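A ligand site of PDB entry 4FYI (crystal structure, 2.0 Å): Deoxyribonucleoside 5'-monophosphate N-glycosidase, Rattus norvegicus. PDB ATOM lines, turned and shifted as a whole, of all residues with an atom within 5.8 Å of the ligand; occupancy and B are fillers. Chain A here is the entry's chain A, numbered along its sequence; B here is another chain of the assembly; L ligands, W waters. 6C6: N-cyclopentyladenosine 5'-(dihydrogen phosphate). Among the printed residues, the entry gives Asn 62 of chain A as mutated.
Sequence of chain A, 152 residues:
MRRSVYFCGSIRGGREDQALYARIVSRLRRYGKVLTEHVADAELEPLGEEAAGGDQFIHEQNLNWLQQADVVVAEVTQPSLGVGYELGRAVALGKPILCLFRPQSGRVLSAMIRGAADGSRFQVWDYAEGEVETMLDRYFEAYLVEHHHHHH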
ATOM      1  N   TYR A   6     -20.675  10.581 -24.249  1.00  0.00           N
ATOM      2  CA  TYR A   6     -19.768  10.620 -23.118  1.00  0.00           C
ATOM      3  C   TYR A   6     -18.751   9.486 -23.285  1.00  0.00           C
ATOM      4  O   TYR A   6     -19.138   8.321 -23.384  1.00  0.00           O
ATOM      5  CB  TYR A   6     -20.585  10.418 -21.836  1.00  0.00           C
ATOM      6  CG  TYR A   6     -19.827  10.600 -20.550  1.00  0.00           C
ATOM      7  CD1 TYR A   6     -19.937  11.782 -19.816  1.00  0.00           C
ATOM      8  CD2 TYR A   6     -18.998   9.584 -20.049  1.00  0.00           C
ATOM      9  CE1 TYR A   6     -19.258  11.958 -18.632  1.00  0.00           C
ATOM     10  CE2 TYR A   6     -18.315   9.765 -18.852  1.00  0.00           C
ATOM     11  CZ  TYR A   6     -18.442  10.947 -18.152  1.00  0.00           C
ATOM     12  OH  TYR A   6     -17.776  11.145 -16.970  1.00  0.00           O
ATOM     13  N   PHE A   7     -17.456   9.807 -23.328  1.00  0.00           N
ATOM     14  CA  PHE A   7     -16.422   8.771 -23.430  1.00  0.00           C
ATOM     15  C   PHE A   7     -15.697   8.517 -22.106  1.00  0.00           C
ATOM     16  O   PHE A   7     -15.270   9.466 -21.456  1.00  0.00           O
ATOM     17  CB  PHE A   7     -15.383   9.106 -24.503  1.00  0.00           C
ATOM     18  CG  PHE A   7     -14.221   8.154 -24.519  1.00  0.00           C
ATOM     19  CD1 PHE A   7     -13.009   8.512 -23.959  1.00  0.00           C
ATOM     20  CD2 PHE A   7     -14.378   6.884 -25.040  1.00  0.00           C
ATOM     21  CE1 PHE A   7     -11.953   7.610 -23.947  1.00  0.00           C
ATOM     22  CE2 PHE A   7     -13.327   5.970 -25.022  1.00  0.00           C
ATOM     23  CZ  PHE A   7     -12.106   6.331 -24.481  1.00  0.00           C
ATOM     24  N   CYS A   8     -15.541   7.237 -21.734  1.00  0.00           N
ATOM     25  CA  CYS A   8     -14.867   6.825 -20.493  1.00  0.00           C
ATOM     26  C   CYS A   8     -13.581   6.046 -20.801  1.00  0.00           C
ATOM     27  O   CYS A   8     -13.580   5.093 -21.591  1.00  0.00           O
ATOM     28  CB  CYS A   8     -15.746   5.901 -19.629  1.00  0.00           C
ATOM     29  SG  CYS A   8     -17.525   6.301 -19.516  1.00  0.00           S
ATOM     30  N   GLY A   9     -12.504   6.430 -20.124  1.00  0.00           N
ATOM     31  CA  GLY A   9     -11.243   5.686 -20.177  1.00  0.00           C
ATOM     32  C   GLY A   9     -10.348   5.992 -18.984  1.00  0.00           C
ATOM     33  O   GLY A   9     -10.359   7.107 -18.450  1.00  0.00           O
ATOM     34  N   SER A  10      -9.575   4.987 -18.568  1.00  0.00           N
ATOM     35  CA  SER A  10      -8.707   5.073 -17.406  1.00  0.00           C
ATOM     36  C   SER A  10      -7.762   6.268 -17.449  1.00  0.00           C
ATOM     37  O   SER A  10      -7.138   6.536 -18.489  1.00  0.00           O
ATOM     38  CB  SER A  10      -7.867   3.801 -17.291  1.00  0.00           C
ATOM     39  OG  SER A  10      -6.973   3.849 -16.189  1.00  0.00           O
ATOM     40  N   ILE A  11      -7.672   6.961 -16.322  1.00  0.00           N
ATOM     41  CA  ILE A  11      -6.661   8.012 -16.109  1.00  0.00           C
ATOM     42  C   ILE A  11      -5.778   7.644 -14.906  1.00  0.00           C
ATOM     43  O   ILE A  11      -4.670   7.139 -15.089  1.00  0.00           O
ATOM     44  CB  ILE A  11      -7.322   9.395 -15.939  1.00  0.00           C
ATOM     45  CG1 ILE A  11      -8.234   9.708 -17.146  1.00  0.00           C
ATOM     46  CG2 ILE A  11      -6.236  10.500 -15.776  1.00  0.00           C
ATOM     47  CD1 ILE A  11      -9.059  11.025 -17.000  1.00  0.00           C
ATOM     48  N   ARG A  12      -6.272   7.828 -13.684  1.00  0.00           N
ATOM     49  CA  ARG A  12      -5.512   7.421 -12.481  1.00  0.00           C
ATOM     50  C   ARG A  12      -5.458   5.903 -12.305  1.00  0.00           C
ATOM     51  O   ARG A  12      -4.656   5.397 -11.515  1.00  0.00           O
ATOM     52  CB  ARG A  12      -6.057   8.094 -11.221  1.00  0.00           C
ATOM     53  CG  ARG A  12      -5.671   9.540 -11.107  1.00  0.00           C
ATOM     54  CD  ARG A  12      -6.132  10.181  -9.804  1.00  0.00           C
ATOM     55  NE  ARG A  12      -5.742  11.594  -9.759  1.00  0.00           N
ATOM     56  CZ  ARG A  12      -6.338  12.541  -9.025  1.00  0.00           C
ATOM     57  NH1 ARG A  12      -7.379  12.265  -8.243  1.00  0.00           N
ATOM     58  NH2 ARG A  12      -5.874  13.782  -9.087  1.00  0.00           N
ATOM     59  N   GLY A  13      -6.299   5.177 -13.036  1.00  0.00           N
ATOM     60  CA  GLY A  13      -6.147   3.735 -13.150  1.00  0.00           C
ATOM     61  C   GLY A  13      -4.904   3.339 -13.936  1.00  0.00           C
ATOM     62  O   GLY A  13      -4.477   2.192 -13.879  1.00  0.00           O
ATOM     63  N   GLY A  14      -4.343   4.290 -14.690  1.00  0.00           N
ATOM     64  CA  GLY A  14      -3.208   4.054 -15.573  1.00  0.00           C
ATOM     65  C   GLY A  14      -3.524   4.617 -16.954  1.00  0.00           C
ATOM     66  O   GLY A  14      -4.639   4.443 -17.441  1.00  0.00           O
ATOM     67  N   THR A  36     -16.946  14.828 -23.136  1.00  0.00           N
ATOM     68  CA  THR A  36     -15.828  14.709 -22.209  1.00  0.00           C
ATOM     69  C   THR A  36     -14.532  15.244 -22.825  1.00  0.00           C
ATOM     70  O   THR A  36     -14.454  15.487 -24.027  1.00  0.00           O
ATOM     71  CB  THR A  36     -15.655  13.245 -21.787  1.00  0.00           C
ATOM     72  OG1 THR A  36     -15.918  12.388 -22.905  1.00  0.00           O
ATOM     73  CG2 THR A  36     -16.610  12.898 -20.661  1.00  0.00           C
ATOM     74  N   ASP A  55     -11.332  17.722  -7.111  1.00  0.00           N
ATOM     75  CA  ASP A  55     -12.005  16.475  -7.474  1.00  0.00           C
ATOM     76  C   ASP A  55     -13.526  16.548  -7.343  1.00  0.00           C
ATOM     77  O   ASP A  55     -14.241  15.906  -8.120  1.00  0.00           O
ATOM     78  CB  ASP A  55     -11.425  15.305  -6.668  1.00  0.00           C
ATOM     79  CG  ASP A  55      -9.945  15.061  -6.974  1.00  0.00           C
ATOM     80  OD1 ASP A  55      -9.332  14.195  -6.328  1.00  0.00           O
ATOM     81  OD2 ASP A  55      -9.390  15.746  -7.878  1.00  0.00           O
ATOM     82  N   ILE A  58     -14.655  18.118 -10.562  1.00  0.00           N
ATOM     83  CA  ILE A  58     -14.514  17.178 -11.669  1.00  0.00           C
ATOM     84  C   ILE A  58     -15.682  16.196 -11.693  1.00  0.00           C
ATOM     85  O   ILE A  58     -16.273  15.939 -12.734  1.00  0.00           O
ATOM     86  CB  ILE A  58     -13.194  16.399 -11.560  1.00  0.00           C
ATOM     87  CG1 ILE A  58     -12.024  17.313 -11.937  1.00  0.00           C
ATOM     88  CG2 ILE A  58     -13.211  15.136 -12.444  1.00  0.00           C
ATOM     89  CD1 ILE A  58     -10.671  16.797 -11.461  1.00  0.00           C
ATOM     90  N   ASN A  62     -18.552  16.003 -14.590  1.00  0.00           N
ATOM     91  CA  ASN A  62     -18.740  14.745 -15.313  1.00  0.00           C
ATOM     92  C   ASN A  62     -20.150  14.196 -15.200  1.00  0.00           C
ATOM     93  O   ASN A  62     -20.711  13.737 -16.197  1.00  0.00           O
ATOM     94  CB  ASN A  62     -17.743  13.689 -14.835  1.00  0.00           C
ATOM     95  CG  ASN A  62     -16.355  13.884 -15.432  1.00  0.00           C
ATOM     96  OD1 ASN A  62     -16.168  14.627 -16.389  1.00  0.00           O
ATOM     97  ND2 ASN A  62     -15.371  13.173 -14.869  1.00  0.00           N
ATOM     98  N   PRO A  79      -8.088  -1.637 -15.918  1.00  0.00           N
ATOM     99  CA  PRO A  79      -8.941  -1.494 -14.737  1.00  0.00           C
ATOM    100  C   PRO A  79      -8.873  -0.083 -14.159  1.00  0.00           C
ATOM    101  O   PRO A  79      -7.775   0.489 -14.055  1.00  0.00           O
ATOM    102  CB  PRO A  79      -8.385  -2.523 -13.771  1.00  0.00           C
ATOM    103  CG  PRO A  79      -7.814  -3.575 -14.651  1.00  0.00           C
ATOM    104  CD  PRO A  79      -7.161  -2.777 -15.763  1.00  0.00           C
ATOM    105  N   SER A  80     -10.041   0.462 -13.797  1.00  0.00           N
ATOM    106  CA  SER A  80     -10.160   1.843 -13.347  1.00  0.00           C
ATOM    107  C   SER A  80     -11.407   2.002 -12.480  1.00  0.00           C
ATOM    108  O   SER A  80     -12.484   1.590 -12.906  1.00  0.00           O
ATOM    109  CB  SER A  80     -10.283   2.785 -14.555  1.00  0.00           C
ATOM    110  OG  SER A  80     -10.882   4.024 -14.151  1.00  0.00           O
ATOM    111  N   LEU A  81     -11.274   2.575 -11.283  1.00  0.00           N
ATOM    112  CA  LEU A  81     -12.434   2.844 -10.441  1.00  0.00           C
ATOM    113  C   LEU A  81     -13.350   3.863 -11.107  1.00  0.00           C
ATOM    114  O   LEU A  81     -14.569   3.751 -11.047  1.00  0.00           O
ATOM    115  CB  LEU A  81     -12.029   3.369  -9.059  1.00  0.00           C
ATOM    116  CG  LEU A  81     -11.334   2.432  -8.091  1.00  0.00           C
ATOM    117  CD1 LEU A  81     -10.716   3.228  -6.922  1.00  0.00           C
ATOM    118  CD2 LEU A  81     -12.274   1.317  -7.576  1.00  0.00           C
ATOM    119  N   GLY A  82     -12.766   4.879 -11.733  1.00  0.00           N
ATOM    120  CA  GLY A  82     -13.545   5.970 -12.298  1.00  0.00           C
ATOM    121  C   GLY A  82     -14.406   5.544 -13.466  1.00  0.00           C
ATOM    122  O   GLY A  82     -15.578   5.940 -13.563  1.00  0.00           O
ATOM    123  N   VAL A  83     -13.824   4.740 -14.356  1.00  0.00           N
ATOM    124  CA  VAL A  83     -14.556   4.203 -15.503  1.00  0.00           C
ATOM    125  C   VAL A  83     -15.680   3.276 -15.021  1.00  0.00           C
ATOM    126  O   VAL A  83     -16.802   3.336 -15.515  1.00  0.00           O
ATOM    127  CB  VAL A  83     -13.631   3.429 -16.466  1.00  0.00           C
ATOM    128  CG1 VAL A  83     -14.452   2.720 -17.561  1.00  0.00           C
ATOM    129  CG2 VAL A  83     -12.584   4.395 -17.098  1.00  0.00           C
ATOM    130  N   GLU A  86     -18.449   5.526 -13.529  1.00  0.00           N
ATOM    131  CA  GLU A  86     -19.186   6.178 -14.612  1.00  0.00           C
ATOM    132  C   GLU A  86     -20.210   5.212 -15.237  1.00  0.00           C
ATOM    133  O   GLU A  86     -21.348   5.597 -15.490  1.00  0.00           O
ATOM    134  CB  GLU A  86     -18.215   6.709 -15.667  1.00  0.00           C
ATOM    135  CG  GLU A  86     -17.436   7.951 -15.214  1.00  0.00           C
ATOM    136  CD  GLU A  86     -16.299   8.336 -16.141  1.00  0.00           C
ATOM    137  OE1 GLU A  86     -16.062   9.551 -16.310  1.00  0.00           O
ATOM    138  OE2 GLU A  86     -15.627   7.449 -16.694  1.00  0.00           O
ATOM    139  N   SER B 110      -8.577   7.831  -7.644  1.00  0.00           N
ATOM    140  CA  SER B 110      -9.505   8.350  -8.651  1.00  0.00           C
ATOM    141  C   SER B 110     -10.248   9.608  -8.212  1.00  0.00           C
ATOM    142  O   SER B 110     -10.868   9.629  -7.153  1.00  0.00           O
ATOM    143  CB  SER B 110     -10.573   7.293  -8.967  1.00  0.00           C
ATOM    144  OG  SER B 110     -11.522   7.784  -9.888  1.00  0.00           O
ATOM    145  N   ALA B 111     -10.220  10.640  -9.047  1.00  0.00           N
ATOM    146  CA  ALA B 111     -10.974  11.873  -8.783  1.00  0.00           C
ATOM    147  C   ALA B 111     -12.483  11.610  -8.700  1.00  0.00           C
ATOM    148  O   ALA B 111     -13.184  12.300  -7.952  1.00  0.00           O
ATOM    149  CB  ALA B 111     -10.673  12.924  -9.851  1.00  0.00           C
ATOM    150  N   MET B 112     -12.973  10.619  -9.448  1.00  0.00           N
ATOM    151  CA  MET B 112     -14.399  10.274  -9.431  1.00  0.00           C
ATOM    152  C   MET B 112     -14.859   9.649  -8.126  1.00  0.00           C
ATOM    153  O   MET B 112     -16.018   9.789  -7.767  1.00  0.00           O
ATOM    154  CB  MET B 112     -14.768   9.336 -10.588  1.00  0.00           C
ATOM    155  CG  MET B 112     -14.704   9.988 -11.950  1.00  0.00           C
ATOM    156  SD  MET B 112     -15.658  11.518 -12.098  1.00  0.00           S
ATOM    157  CE  MET B 112     -17.336  10.898 -12.244  1.00  0.00           C
HETATM  158  C65 6C6 L   1      -7.582  15.168 -11.860  1.00  0.00           C
HETATM  159  C64 6C6 L   1      -6.112  15.238 -12.291  1.00  0.00           C
HETATM  160  C63 6C6 L   1      -5.981  14.350 -13.529  1.00  0.00           C
HETATM  161  C62 6C6 L   1      -7.113  13.332 -13.383  1.00  0.00           C
HETATM  162  C61 6C6 L   1      -8.269  14.107 -12.744  1.00  0.00           C
HETATM  163  N6  6C6 L   1      -9.055  14.802 -13.777  1.00  0.00           N
HETATM  164  C6  6C6 L   1     -10.119  14.303 -14.439  1.00  0.00           C
HETATM  165  N1  6C6 L   1     -10.773  15.104 -15.301  1.00  0.00           N
HETATM  166  C2  6C6 L   1     -11.824  14.686 -15.991  1.00  0.00           C
HETATM  167  N3  6C6 L   1     -12.307  13.466 -15.845  1.00  0.00           N
HETATM  168  C4  6C6 L   1     -11.710  12.602 -14.991  1.00  0.00           C
HETATM  169  C5  6C6 L   1     -10.601  13.006 -14.261  1.00  0.00           C
HETATM  170  N7  6C6 L   1     -10.248  11.973 -13.511  1.00  0.00           N
HETATM  171  C8  6C6 L   1     -11.082  10.967 -13.753  1.00  0.00           C
HETATM  172  N9  6C6 L   1     -11.982  11.346 -14.656  1.00  0.00           N
HETATM  173  C1' 6C6 L   1     -13.102  10.531 -15.240  1.00  0.00           C
HETATM  174  O4' 6C6 L   1     -13.153   9.183 -14.697  1.00  0.00           O
HETATM  175  C2' 6C6 L   1     -12.896  10.406 -16.762  1.00  0.00           C
HETATM  176  O2' 6C6 L   1     -14.106  10.731 -17.471  1.00  0.00           O
HETATM  177  C3' 6C6 L   1     -12.438   8.962 -16.998  1.00  0.00           C
HETATM  178  O3' 6C6 L   1     -13.278   8.280 -17.962  1.00  0.00           O
HETATM  179  C4' 6C6 L   1     -12.554   8.256 -15.641  1.00  0.00           C
HETATM  180  C5' 6C6 L   1     -11.141   7.864 -15.184  1.00  0.00           C
HETATM  181  O5' 6C6 L   1     -11.138   7.381 -13.866  1.00  0.00           O
HETATM  182  PA  6C6 L   1      -9.745   6.975 -13.110  1.00  0.00           P
HETATM  183  OA2 6C6 L   1     -10.199   6.418 -11.720  1.00  0.00           O
HETATM  184  OA3 6C6 L   1      -9.010   8.353 -12.894  1.00  0.00           O
HETATM  185  OA1 6C6 L   1      -9.003   5.968 -13.931  1.00  0.00           O
HETATM  186  O   HOH W   1      -8.810  10.484 -11.524  1.00  0.00           O
HETATM  187  O   HOH W   2      -8.800   4.134 -10.675  1.00  0.00           O
HETATM  188  O   HOH W   3     -10.544  17.594 -16.188  1.00  0.00           O
HETATM  189  O   HOH W   4     -13.160  10.592 -20.034  1.00  0.00           O
HETATM  190  O   HOH W   5     -14.572  13.476 -18.445  1.00  0.00           O
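Water W1 lies within hydrogen-bond range of an oxygen (OA3) of the ligand (2.5 Å) and the backbone NH of Ala 111 of chain B (2.9 Å).
Water W4 lies within hydrogen-bond range of O2' of the ligand (2.7 Å) and O of Phe 7 (2.8 Å).
Water W2 lies within hydrogen-bond range of OA2 of the ligand (2.9 Å) and N of Leu 81 (3.0 Å).
Water W5 lies within hydrogen-bond range of OD1 of Asn 62 (2.8 Å) and O2' of the ligand (2.9 Å).
OE2 of Glu 86 lies close to SG of Cys 8, at 3.6 Å.
OG of Ser 110 of chain B sits close to N of Met 112 of chain B, at 3.2 Å.
The side-chain hydroxyl (OG) of Ser 80 sits at hydrogen-bond distance from the backbone NH (N) of Gly 82 (3.2 Å).
The backbone NH (N) of Val 83 sits at hydrogen-bond distance from the side-chain hydroxyl (OG) of Ser 80 (3.0 Å).
NH1 of Arg 12 lies within salt-bridge range of OD1 of Asp 55 (3.3 Å).
The side-chain hydroxyl (OG) of Ser 10 sits close to the backbone NH (N) of Gly 13 (3.5 Å).
The side-chain amide nitrogen of Asn 62 lies within hydrogen-bond range of the side-chain sulfur of Met 112 of chain B.
The side-chain hydroxyl (OG) of Ser 10 is in hydrogen-bond range of the backbone carbonyl oxygen (O) of Gly 14 (2.7 Å).
Tyr 6 touches the ligand (OH to O2', 3.7 Å).
Cys 8 touches the ligand (CA to O3', 3.3 Å).
CA of Ser 10 touches OA1 of the ligand (3.6 Å).
CD1 of Ile 58 touches N6 of the ligand, 3.5 Å away.
Val 83 touches the ligand (N to O5', 3.8 Å).
Ala 111 of chain B touches the ligand (CB to N7, 3.8 Å).
CG of Met 112 of chain B touches O4' of the ligand, at 3.3 Å.
Hydrophobic or aromatic side chains within 4 Å of the ligand: Ile 11, Ile 58, Ala 111 of chain B and Met 112 of chain B.
16 residues have an atom within 4 Å of the ligand: Tyr 6, Cys 8, Gly 9, Ser 10, Ile 11, Arg 12, Gly 13, Ile 58, Asn 62, Ser 80, Gly 82, Val 83, Glu 86, Ser 110 of chain B, Ala 111 of chain B and Met 112 of chain B.
The side-chain carboxylate (OE1) of Glu 86 is in hydrogen-bond range of an oxygen (O2') of the ligand (2.6 Å).
The side-chain hydroxyl of Ser 110 of chain B sits at hydrogen-bond distance from an oxygen (OA2) of the ligand (2.6 Å).
The side-chain hydroxyl of Ser 80 lies within hydrogen-bond range of an oxygen (OA1) of the ligand, at 2.7 Å.
The backbone NH (N) of Arg 12 is in hydrogen-bond range of an oxygen (OA3) of the ligand (2.9 Å).
The backbone NH (N) of Ile 11 is in hydrogen-bond range of an oxygen (OA1) of the ligand.
N of Gly 9 sits at hydrogen-bond distance from O3' of the ligand (2.9 Å).
The backbone carbonyl oxygen (O) of Gly 9 sits close to an oxygen (O3') of the ligand.
An oxygen (OA1) of the ligand lies within hydrogen-bond range of the backbone NH of Gly 13.
An oxygen (OA2) of the ligand lies within hydrogen-bond range of the backbone NH (N) of Gly 82, 3.0 Å away.
N3 of the ligand sits at hydrogen-bond distance from ND2 of Asn 62 (3.2 Å).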
